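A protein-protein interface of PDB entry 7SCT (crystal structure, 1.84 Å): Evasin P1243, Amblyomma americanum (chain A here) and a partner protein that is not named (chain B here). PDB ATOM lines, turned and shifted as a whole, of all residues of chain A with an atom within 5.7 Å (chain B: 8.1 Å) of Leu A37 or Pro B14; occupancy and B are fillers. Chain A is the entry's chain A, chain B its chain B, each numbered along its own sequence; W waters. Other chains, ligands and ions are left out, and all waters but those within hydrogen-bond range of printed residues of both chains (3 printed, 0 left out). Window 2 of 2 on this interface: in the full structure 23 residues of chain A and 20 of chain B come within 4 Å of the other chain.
Printed residues of chain B within 4 Å of His A28: Ser B15 (2.9 Å) and Cys B17 (3.5 Å).
Of the printed residues of chain B, Leu A37 touches Pro B14 and Cys B17.
Of the printed residues of chain B, Tyr A57 touches Cys B18 (3.9 Å) and His B41 (3.5 Å).
Pro B14 touches one residue of chain A.
Thr B16 touches none of the printed residues of chain A.
The nearest residue of chain B that does not touch Leu A37 is Ser B15 (4.2 Å).
The nearest residue of chain A that does not touch Pro B14 is Asn A30 (5.6 Å).
The nearest printed residue of chain A that does not touch His B41 is Leu A37 (4.7 Å).
Water W1 lies within hydrogen-bond range of O of Leu A37 (2.6 Å), N of His B41 (2.9 Å) and OH of Tyr A57 (3.3 Å).
Water W3 bridges the backbone carbonyl oxygen of Asn B39 (2.7 Å) and the backbone NH of Leu A37 (3.2 Å).
Water W2 lies within hydrogen-bond range of O of Cys B18 (2.7 Å), N of Leu B42 (2.8 Å), OH of Tyr A57 (2.8 Å) and N of His B41 (3.2 Å).
The backbone NH (N) of His A28 sits at hydrogen-bond distance from the backbone carbonyl oxygen (O) of Ser B15, 2.9 Å away.
Hydrophobic or aromatic side chains of chain A that line the printed part of chain B: His A28, Val A36, Leu A37, Tyr A57 and Pro A58.
Printed residues of chain B that touch a printed residue of chain A: Pro B14, Ser B15, Cys B17, Cys B18 and His B41.
Among the printed residues, 8 pairs touch across the chains.
Among the printed residues, no Asp or Glu carboxylate lies within 4 Å of a Lys or Arg side-chain nitrogen of the other chain.
Cys B17 touches His A28 (CB to CE1, 3.5 Å).
Val A36 touches His B41.
O of Pro B14 touches CD1 of Leu A37 (3.7 Å).
Cys B17 touches Leu A37 (SG to CD1, 3.9 Å).
OH of Tyr A57 touches O of Cys B18 (3.9 Å).
Tyr A57 touches His B41 (CE1 to CD2, 3.5 Å).
CD of Pro A58 touches CG of His B41, 3.5 Å away.
The side-chain hydroxyl (OH) of Tyr A57 lies within hydrogen-bond range of a ring nitrogen (NE2) of His A28, 2.5 Å away.
The side-chain amide nitrogen (ND2) of Asn A31 lies within hydrogen-bond range of the backbone carbonyl oxygen (O) of Val A36.
The backbone carbonyl oxygen (O) of Val A36 sits at hydrogen-bond distance from the side-chain amino group (NZ) of Lys A38.
N of Leu A39 lies within hydrogen-bond range of O of Pro A58 (3.1 Å).
The side-chain sulfur of Cys B40 is disulfide-bonded to the side-chain sulfur of Cys B17 (2.1 Å).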
ATOM      1  N   HIS A  28      23.009   9.985  -0.944  1.00  0.00           N
ATOM      2  CA  HIS A  28      22.003  10.880  -0.376  1.00  0.00           C
ATOM      3  C   HIS A  28      22.092  12.247  -1.048  1.00  0.00           C
ATOM      4  O   HIS A  28      23.074  12.573  -1.715  1.00  0.00           O
ATOM      5  CB  HIS A  28      22.198  11.048   1.145  1.00  0.00           C
ATOM      6  CG  HIS A  28      21.786   9.857   1.954  1.00  0.00           C
ATOM      7  ND1 HIS A  28      22.208   8.577   1.665  1.00  0.00           N
ATOM      8  CD2 HIS A  28      20.956   9.749   3.023  1.00  0.00           C
ATOM      9  CE1 HIS A  28      21.666   7.732   2.528  1.00  0.00           C
ATOM     10  NE2 HIS A  28      20.898   8.417   3.360  1.00  0.00           N
ATOM     11  N   LEU A  29      21.069  13.071  -0.840  1.00  0.00           N
ATOM     12  CA  LEU A  29      21.135  14.455  -1.294  1.00  0.00           C
ATOM     13  C   LEU A  29      21.700  15.325  -0.177  1.00  0.00           C
ATOM     14  O   LEU A  29      21.507  15.039   1.005  1.00  0.00           O
ATOM     15  CB  LEU A  29      19.759  14.966  -1.729  1.00  0.00           C
ATOM     16  CG  LEU A  29      19.184  14.331  -3.014  1.00  0.00           C
ATOM     17  CD1 LEU A  29      17.846  14.943  -3.379  1.00  0.00           C
ATOM     18  CD2 LEU A  29      20.138  14.478  -4.168  1.00  0.00           C
ATOM     19  N   ASN A  30      22.421  16.379  -0.555  1.00  0.00           N
ATOM     20  CA  ASN A  30      22.996  17.248   0.460  1.00  0.00           C
ATOM     21  C   ASN A  30      22.108  18.478   0.637  1.00  0.00           C
ATOM     22  O   ASN A  30      21.148  18.697  -0.114  1.00  0.00           O
ATOM     23  CB  ASN A  30      24.427  17.658   0.098  1.00  0.00           C
ATOM     24  CG  ASN A  30      25.284  17.926   1.339  1.00  0.00           C
ATOM     25  OD1 ASN A  30      24.908  18.702   2.227  1.00  0.00           O
ATOM     26  ND2 ASN A  30      26.451  17.283   1.397  1.00  0.00           N
ATOM     27  N   ASN A  31      22.438  19.290   1.645  1.00  0.00           N
ATOM     28  CA  ASN A  31      21.615  20.448   1.969  1.00  0.00           C
ATOM     29  C   ASN A  31      22.513  21.575   2.457  1.00  0.00           C
ATOM     30  O   ASN A  31      23.677  21.361   2.810  1.00  0.00           O
ATOM     31  CB  ASN A  31      20.560  20.100   3.022  1.00  0.00           C
ATOM     32  CG  ASN A  31      21.180  19.571   4.301  1.00  0.00           C
ATOM     33  OD1 ASN A  31      21.744  20.337   5.076  1.00  0.00           O
ATOM     34  ND2 ASN A  31      21.113  18.261   4.510  1.00  0.00           N
ATOM     35  N   THR A  35      21.642  20.107   8.443  1.00  0.00           N
ATOM     36  CA  THR A  35      20.882  18.990   8.971  1.00  0.00           C
ATOM     37  C   THR A  35      21.316  17.673   8.326  1.00  0.00           C
ATOM     38  O   THR A  35      22.108  17.628   7.377  1.00  0.00           O
ATOM     39  CB  THR A  35      19.381  19.210   8.760  1.00  0.00           C
ATOM     40  OG1 THR A  35      19.100  19.263   7.359  1.00  0.00           O
ATOM     41  CG2 THR A  35      18.928  20.507   9.409  1.00  0.00           C
ATOM     42  N   VAL A  36      20.744  16.588   8.846  1.00  0.00           N
ATOM     43  CA  VAL A  36      21.117  15.250   8.418  1.00  0.00           C
ATOM     44  C   VAL A  36      20.920  15.088   6.900  1.00  0.00           C
ATOM     45  O   VAL A  36      20.014  15.675   6.298  1.00  0.00           O
ATOM     46  CB  VAL A  36      20.281  14.223   9.197  1.00  0.00           C
ATOM     47  CG1 VAL A  36      18.808  14.345   8.785  1.00  0.00           C
ATOM     48  CG2 VAL A  36      20.783  12.820   8.957  1.00  0.00           C
ATOM     49  N   LEU A  37      21.803  14.307   6.277  1.00  0.00           N
ATOM     50  CA  LEU A  37      21.642  13.960   4.863  1.00  0.00           C
ATOM     51  C   LEU A  37      20.419  13.084   4.672  1.00  0.00           C
ATOM     52  O   LEU A  37      20.189  12.156   5.453  1.00  0.00           O
ATOM     53  CB  LEU A  37      22.867  13.200   4.366  1.00  0.00           C
ATOM     54  CG  LEU A  37      24.195  13.936   4.317  1.00  0.00           C
ATOM     55  CD1 LEU A  37      25.300  12.996   3.821  1.00  0.00           C
ATOM     56  CD2 LEU A  37      24.077  15.165   3.427  1.00  0.00           C
ATOM     57  N   LYS A  38      19.668  13.329   3.582  1.00  0.00           N
ATOM     58  CA  LYS A  38      18.386  12.669   3.355  1.00  0.00           C
ATOM     59  C   LYS A  38      18.372  11.930   2.025  1.00  0.00           C
ATOM     60  O   LYS A  38      19.006  12.342   1.051  1.00  0.00           O
ATOM     61  CB  LYS A  38      17.234  13.693   3.409  1.00  0.00           C
ATOM     62  CG  LYS A  38      17.398  14.663   4.600  1.00  0.00           C
ATOM     63  CD  LYS A  38      16.110  15.427   4.928  1.00  0.00           C
ATOM     64  CE  LYS A  38      16.210  16.212   6.241  1.00  0.00           C
ATOM     65  NZ  LYS A  38      17.492  17.000   6.378  1.00  0.00           N
ATOM     66  N   LEU A  39      17.634  10.827   2.000  1.00  0.00           N
ATOM     67  CA  LEU A  39      17.478  10.031   0.796  1.00  0.00           C
ATOM     68  C   LEU A  39      16.480  10.689  -0.145  1.00  0.00           C
ATOM     69  O   LEU A  39      15.467  11.229   0.292  1.00  0.00           O
ATOM     70  CB  LEU A  39      16.991   8.623   1.144  1.00  0.00           C
ATOM     71  CG  LEU A  39      17.155   7.555   0.066  1.00  0.00           C
ATOM     72  CD1 LEU A  39      18.626   7.243  -0.108  1.00  0.00           C
ATOM     73  CD2 LEU A  39      16.384   6.301   0.458  1.00  0.00           C
ATOM     74  N   TYR A  57      12.995   7.006   8.291  1.00  0.00           N
ATOM     75  CA  TYR A  57      14.224   7.484   7.656  1.00  0.00           C
ATOM     76  C   TYR A  57      13.980   8.842   7.005  1.00  0.00           C
ATOM     77  O   TYR A  57      12.924   9.055   6.397  1.00  0.00           O
ATOM     78  CB  TYR A  57      14.731   6.482   6.597  1.00  0.00           C
ATOM     79  CG  TYR A  57      16.184   6.738   6.279  1.00  0.00           C
ATOM     80  CD1 TYR A  57      17.171   6.171   7.055  1.00  0.00           C
ATOM     81  CD2 TYR A  57      16.554   7.611   5.262  1.00  0.00           C
ATOM     82  CE1 TYR A  57      18.506   6.432   6.829  1.00  0.00           C
ATOM     83  CE2 TYR A  57      17.899   7.890   5.025  1.00  0.00           C
ATOM     84  CZ  TYR A  57      18.860   7.287   5.799  1.00  0.00           C
ATOM     85  OH  TYR A  57      20.194   7.577   5.601  1.00  0.00           O
ATOM     86  N   PRO A  58      14.929   9.777   7.098  1.00  0.00           N
ATOM     87  CA  PRO A  58      14.706  11.113   6.520  1.00  0.00           C
ATOM     88  C   PRO A  58      14.791  11.088   5.003  1.00  0.00           C
ATOM     89  O   PRO A  58      15.711  10.509   4.435  1.00  0.00           O
ATOM     90  CB  PRO A  58      15.854  11.949   7.096  1.00  0.00           C
ATOM     91  CG  PRO A  58      16.932  10.930   7.372  1.00  0.00           C
ATOM     92  CD  PRO A  58      16.184   9.710   7.872  1.00  0.00           C
ATOM     93  N   PRO B  14      30.760  13.722   2.074  1.00  0.00           N
ATOM     94  CA  PRO B  14      30.673  12.271   2.283  1.00  0.00           C
ATOM     95  C   PRO B  14      29.253  11.769   2.058  1.00  0.00           C
ATOM     96  O   PRO B  14      28.548  11.421   3.020  1.00  0.00           O
ATOM     97  CB  PRO B  14      31.103  12.098   3.747  1.00  0.00           C
ATOM     98  CG  PRO B  14      30.961  13.479   4.359  1.00  0.00           C
ATOM     99  CD  PRO B  14      31.328  14.405   3.247  1.00  0.00           C
ATOM    100  N   SER B  15      28.850  11.720   0.785  1.00  0.00           N
ATOM    101  CA  SER B  15      27.437  11.676   0.419  1.00  0.00           C
ATOM    102  C   SER B  15      26.797  10.299   0.541  1.00  0.00           C
ATOM    103  O   SER B  15      25.586  10.193   0.307  1.00  0.00           O
ATOM    104  CB  SER B  15      27.245  12.180  -1.017  1.00  0.00           C
ATOM    105  N   THR B  16      27.537   9.247   0.887  1.00  0.00           N
ATOM    106  CA  THR B  16      26.951   7.913   0.933  1.00  0.00           C
ATOM    107  C   THR B  16      26.840   7.423   2.372  1.00  0.00           C
ATOM    108  O   THR B  16      27.823   7.409   3.120  1.00  0.00           O
ATOM    109  CB  THR B  16      27.728   6.923   0.060  1.00  0.00           C
ATOM    110  OG1 THR B  16      28.914   6.506   0.730  1.00  0.00           O
ATOM    111  CG2 THR B  16      28.082   7.567  -1.287  1.00  0.00           C
ATOM    112  N   CYS B  17      25.632   7.024   2.744  1.00  0.00           N
ATOM    113  CA  CYS B  17      25.280   6.704   4.115  1.00  0.00           C
ATOM    114  C   CYS B  17      24.518   5.392   4.130  1.00  0.00           C
ATOM    115  O   CYS B  17      23.850   5.045   3.159  1.00  0.00           O
ATOM    116  CB  CYS B  17      24.386   7.799   4.734  1.00  0.00           C
ATOM    117  SG  CYS B  17      25.243   9.322   5.161  1.00  0.00           S
ATOM    118  N   CYS B  18      24.579   4.701   5.267  1.00  0.00           N
ATOM    119  CA  CYS B  18      23.940   3.405   5.461  1.00  0.00           C
ATOM    120  C   CYS B  18      22.507   3.559   5.959  1.00  0.00           C
ATOM    121  O   CYS B  18      22.211   4.473   6.727  1.00  0.00           O
ATOM    122  CB  CYS B  18      24.730   2.605   6.492  1.00  0.00           C
ATOM    123  SG  CYS B  18      26.352   2.193   5.857  1.00  0.00           S
ATOM    124  N   LYS B  36      34.652   4.890   7.187  1.00  0.00           N
ATOM    125  CA  LYS B  36      33.712   5.379   8.184  1.00  0.00           C
ATOM    126  C   LYS B  36      32.636   6.239   7.540  1.00  0.00           C
ATOM    127  O   LYS B  36      32.894   7.039   6.631  1.00  0.00           O
ATOM    128  CB  LYS B  36      34.385   6.164   9.303  1.00  0.00           C
ATOM    129  CG  LYS B  36      35.266   5.265  10.175  1.00  0.00           C
ATOM    130  CD  LYS B  36      35.884   6.035  11.303  1.00  0.00           C
ATOM    131  CE  LYS B  36      36.724   5.084  12.106  1.00  0.00           C
ATOM    132  NZ  LYS B  36      37.385   5.712  13.252  1.00  0.00           N
ATOM    133  N   ALA B  37      31.412   6.044   8.012  1.00  0.00           N
ATOM    134  CA  ALA B  37      30.263   6.793   7.516  1.00  0.00           C
ATOM    135  C   ALA B  37      29.444   7.213   8.734  1.00  0.00           C
ATOM    136  O   ALA B  37      28.272   6.877   8.875  1.00  0.00           O
ATOM    137  CB  ALA B  37      29.433   5.968   6.539  1.00  0.00           C
ATOM    138  N   LEU B  38      30.101   7.936   9.645  1.00  0.00           N
ATOM    139  CA  LEU B  38      29.478   8.281  10.920  1.00  0.00           C
ATOM    140  C   LEU B  38      28.623   9.539  10.844  1.00  0.00           C
ATOM    141  O   LEU B  38      27.757   9.736  11.702  1.00  0.00           O
ATOM    142  CB  LEU B  38      30.538   8.466  12.016  1.00  0.00           C
ATOM    143  CG  LEU B  38      31.432   7.246  12.240  1.00  0.00           C
ATOM    144  CD1 LEU B  38      32.536   7.561  13.249  1.00  0.00           C
ATOM    145  CD2 LEU B  38      30.615   6.044  12.666  1.00  0.00           C
ATOM    146  N   ASN B  39      28.841  10.399   9.859  1.00  0.00           N
ATOM    147  CA  ASN B  39      28.111  11.662   9.805  1.00  0.00           C
ATOM    148  C   ASN B  39      26.836  11.472   8.976  1.00  0.00           C
ATOM    149  O   ASN B  39      26.603  12.133   7.966  1.00  0.00           O
ATOM    150  CB  ASN B  39      29.001  12.755   9.235  1.00  0.00           C
ATOM    151  CG  ASN B  39      28.486  14.145   9.531  1.00  0.00           C
ATOM    152  OD1 ASN B  39      27.620  14.342  10.386  1.00  0.00           O
ATOM    153  ND2 ASN B  39      29.014  15.127   8.809  1.00  0.00           N
ATOM    154  N   CYS B  40      26.003  10.544   9.451  1.00  0.00           N
ATOM    155  CA  CYS B  40      24.832  10.056   8.728  1.00  0.00           C
ATOM    156  C   CYS B  40      23.693   9.851   9.712  1.00  0.00           C
ATOM    157  O   CYS B  40      23.913   9.769  10.913  1.00  0.00           O
ATOM    158  CB  CYS B  40      25.127   8.724   8.045  1.00  0.00           C
ATOM    159  SG  CYS B  40      26.411   8.837   6.811  1.00  0.00           S
ATOM    160  N   HIS B  41      22.474   9.715   9.183  1.00  0.00           N
ATOM    161  CA  HIS B  41      21.332   9.412  10.043  1.00  0.00           C
ATOM    162  C   HIS B  41      21.565   8.123  10.813  1.00  0.00           C
ATOM    163  O   HIS B  41      21.239   8.033  12.001  1.00  0.00           O
ATOM    164  CB  HIS B  41      20.053   9.298   9.209  1.00  0.00           C
ATOM    165  CG  HIS B  41      18.842   8.934  10.015  1.00  0.00           C
ATOM    166  ND1 HIS B  41      18.228   9.822  10.876  1.00  0.00           N
ATOM    167  CD2 HIS B  41      18.121   7.788  10.083  1.00  0.00           C
ATOM    168  CE1 HIS B  41      17.185   9.238  11.443  1.00  0.00           C
ATOM    169  NE2 HIS B  41      17.109   7.997  10.994  1.00  0.00           N
ATOM    170  N   LEU B  42      22.124   7.106  10.146  1.00  0.00           N
ATOM    171  CA  LEU B  42      22.488   5.841  10.792  1.00  0.00           C
ATOM    172  C   LEU B  42      24.002   5.717  10.722  1.00  0.00           C
ATOM    173  O   LEU B  42      24.541   5.263   9.700  1.00  0.00           O
ATOM    174  CB  LEU B  42      21.827   4.650  10.103  1.00  0.00           C
ATOM    175  CG  LEU B  42      22.004   3.325  10.840  1.00  0.00           C
ATOM    176  CD1 LEU B  42      21.139   3.304  12.113  1.00  0.00           C
ATOM    177  CD2 LEU B  42      21.674   2.156   9.909  1.00  0.00           C
ATOM    178  N   THR B  78      37.794   6.660  -0.094  1.00  0.00           N
ATOM    179  CA  THR B  78      36.622   6.494  -0.946  1.00  0.00           C
ATOM    180  C   THR B  78      36.999   6.616  -2.427  1.00  0.00           C
ATOM    181  O   THR B  78      37.716   7.538  -2.832  1.00  0.00           O
ATOM    182  CB  THR B  78      35.516   7.515  -0.587  1.00  0.00           C
ATOM    183  OG1 THR B  78      36.081   8.830  -0.487  1.00  0.00           O
ATOM    184  CG2 THR B  78      34.843   7.143   0.735  1.00  0.00           C
HETATM  185  O   HOH W   1      21.779  10.329   6.485  1.00  0.00           O
HETATM  186  O   HOH W   2      22.369   7.104   7.375  1.00  0.00           O
HETATM  187  O   HOH W   3      24.368  13.667   8.070  1.00  0.00           O
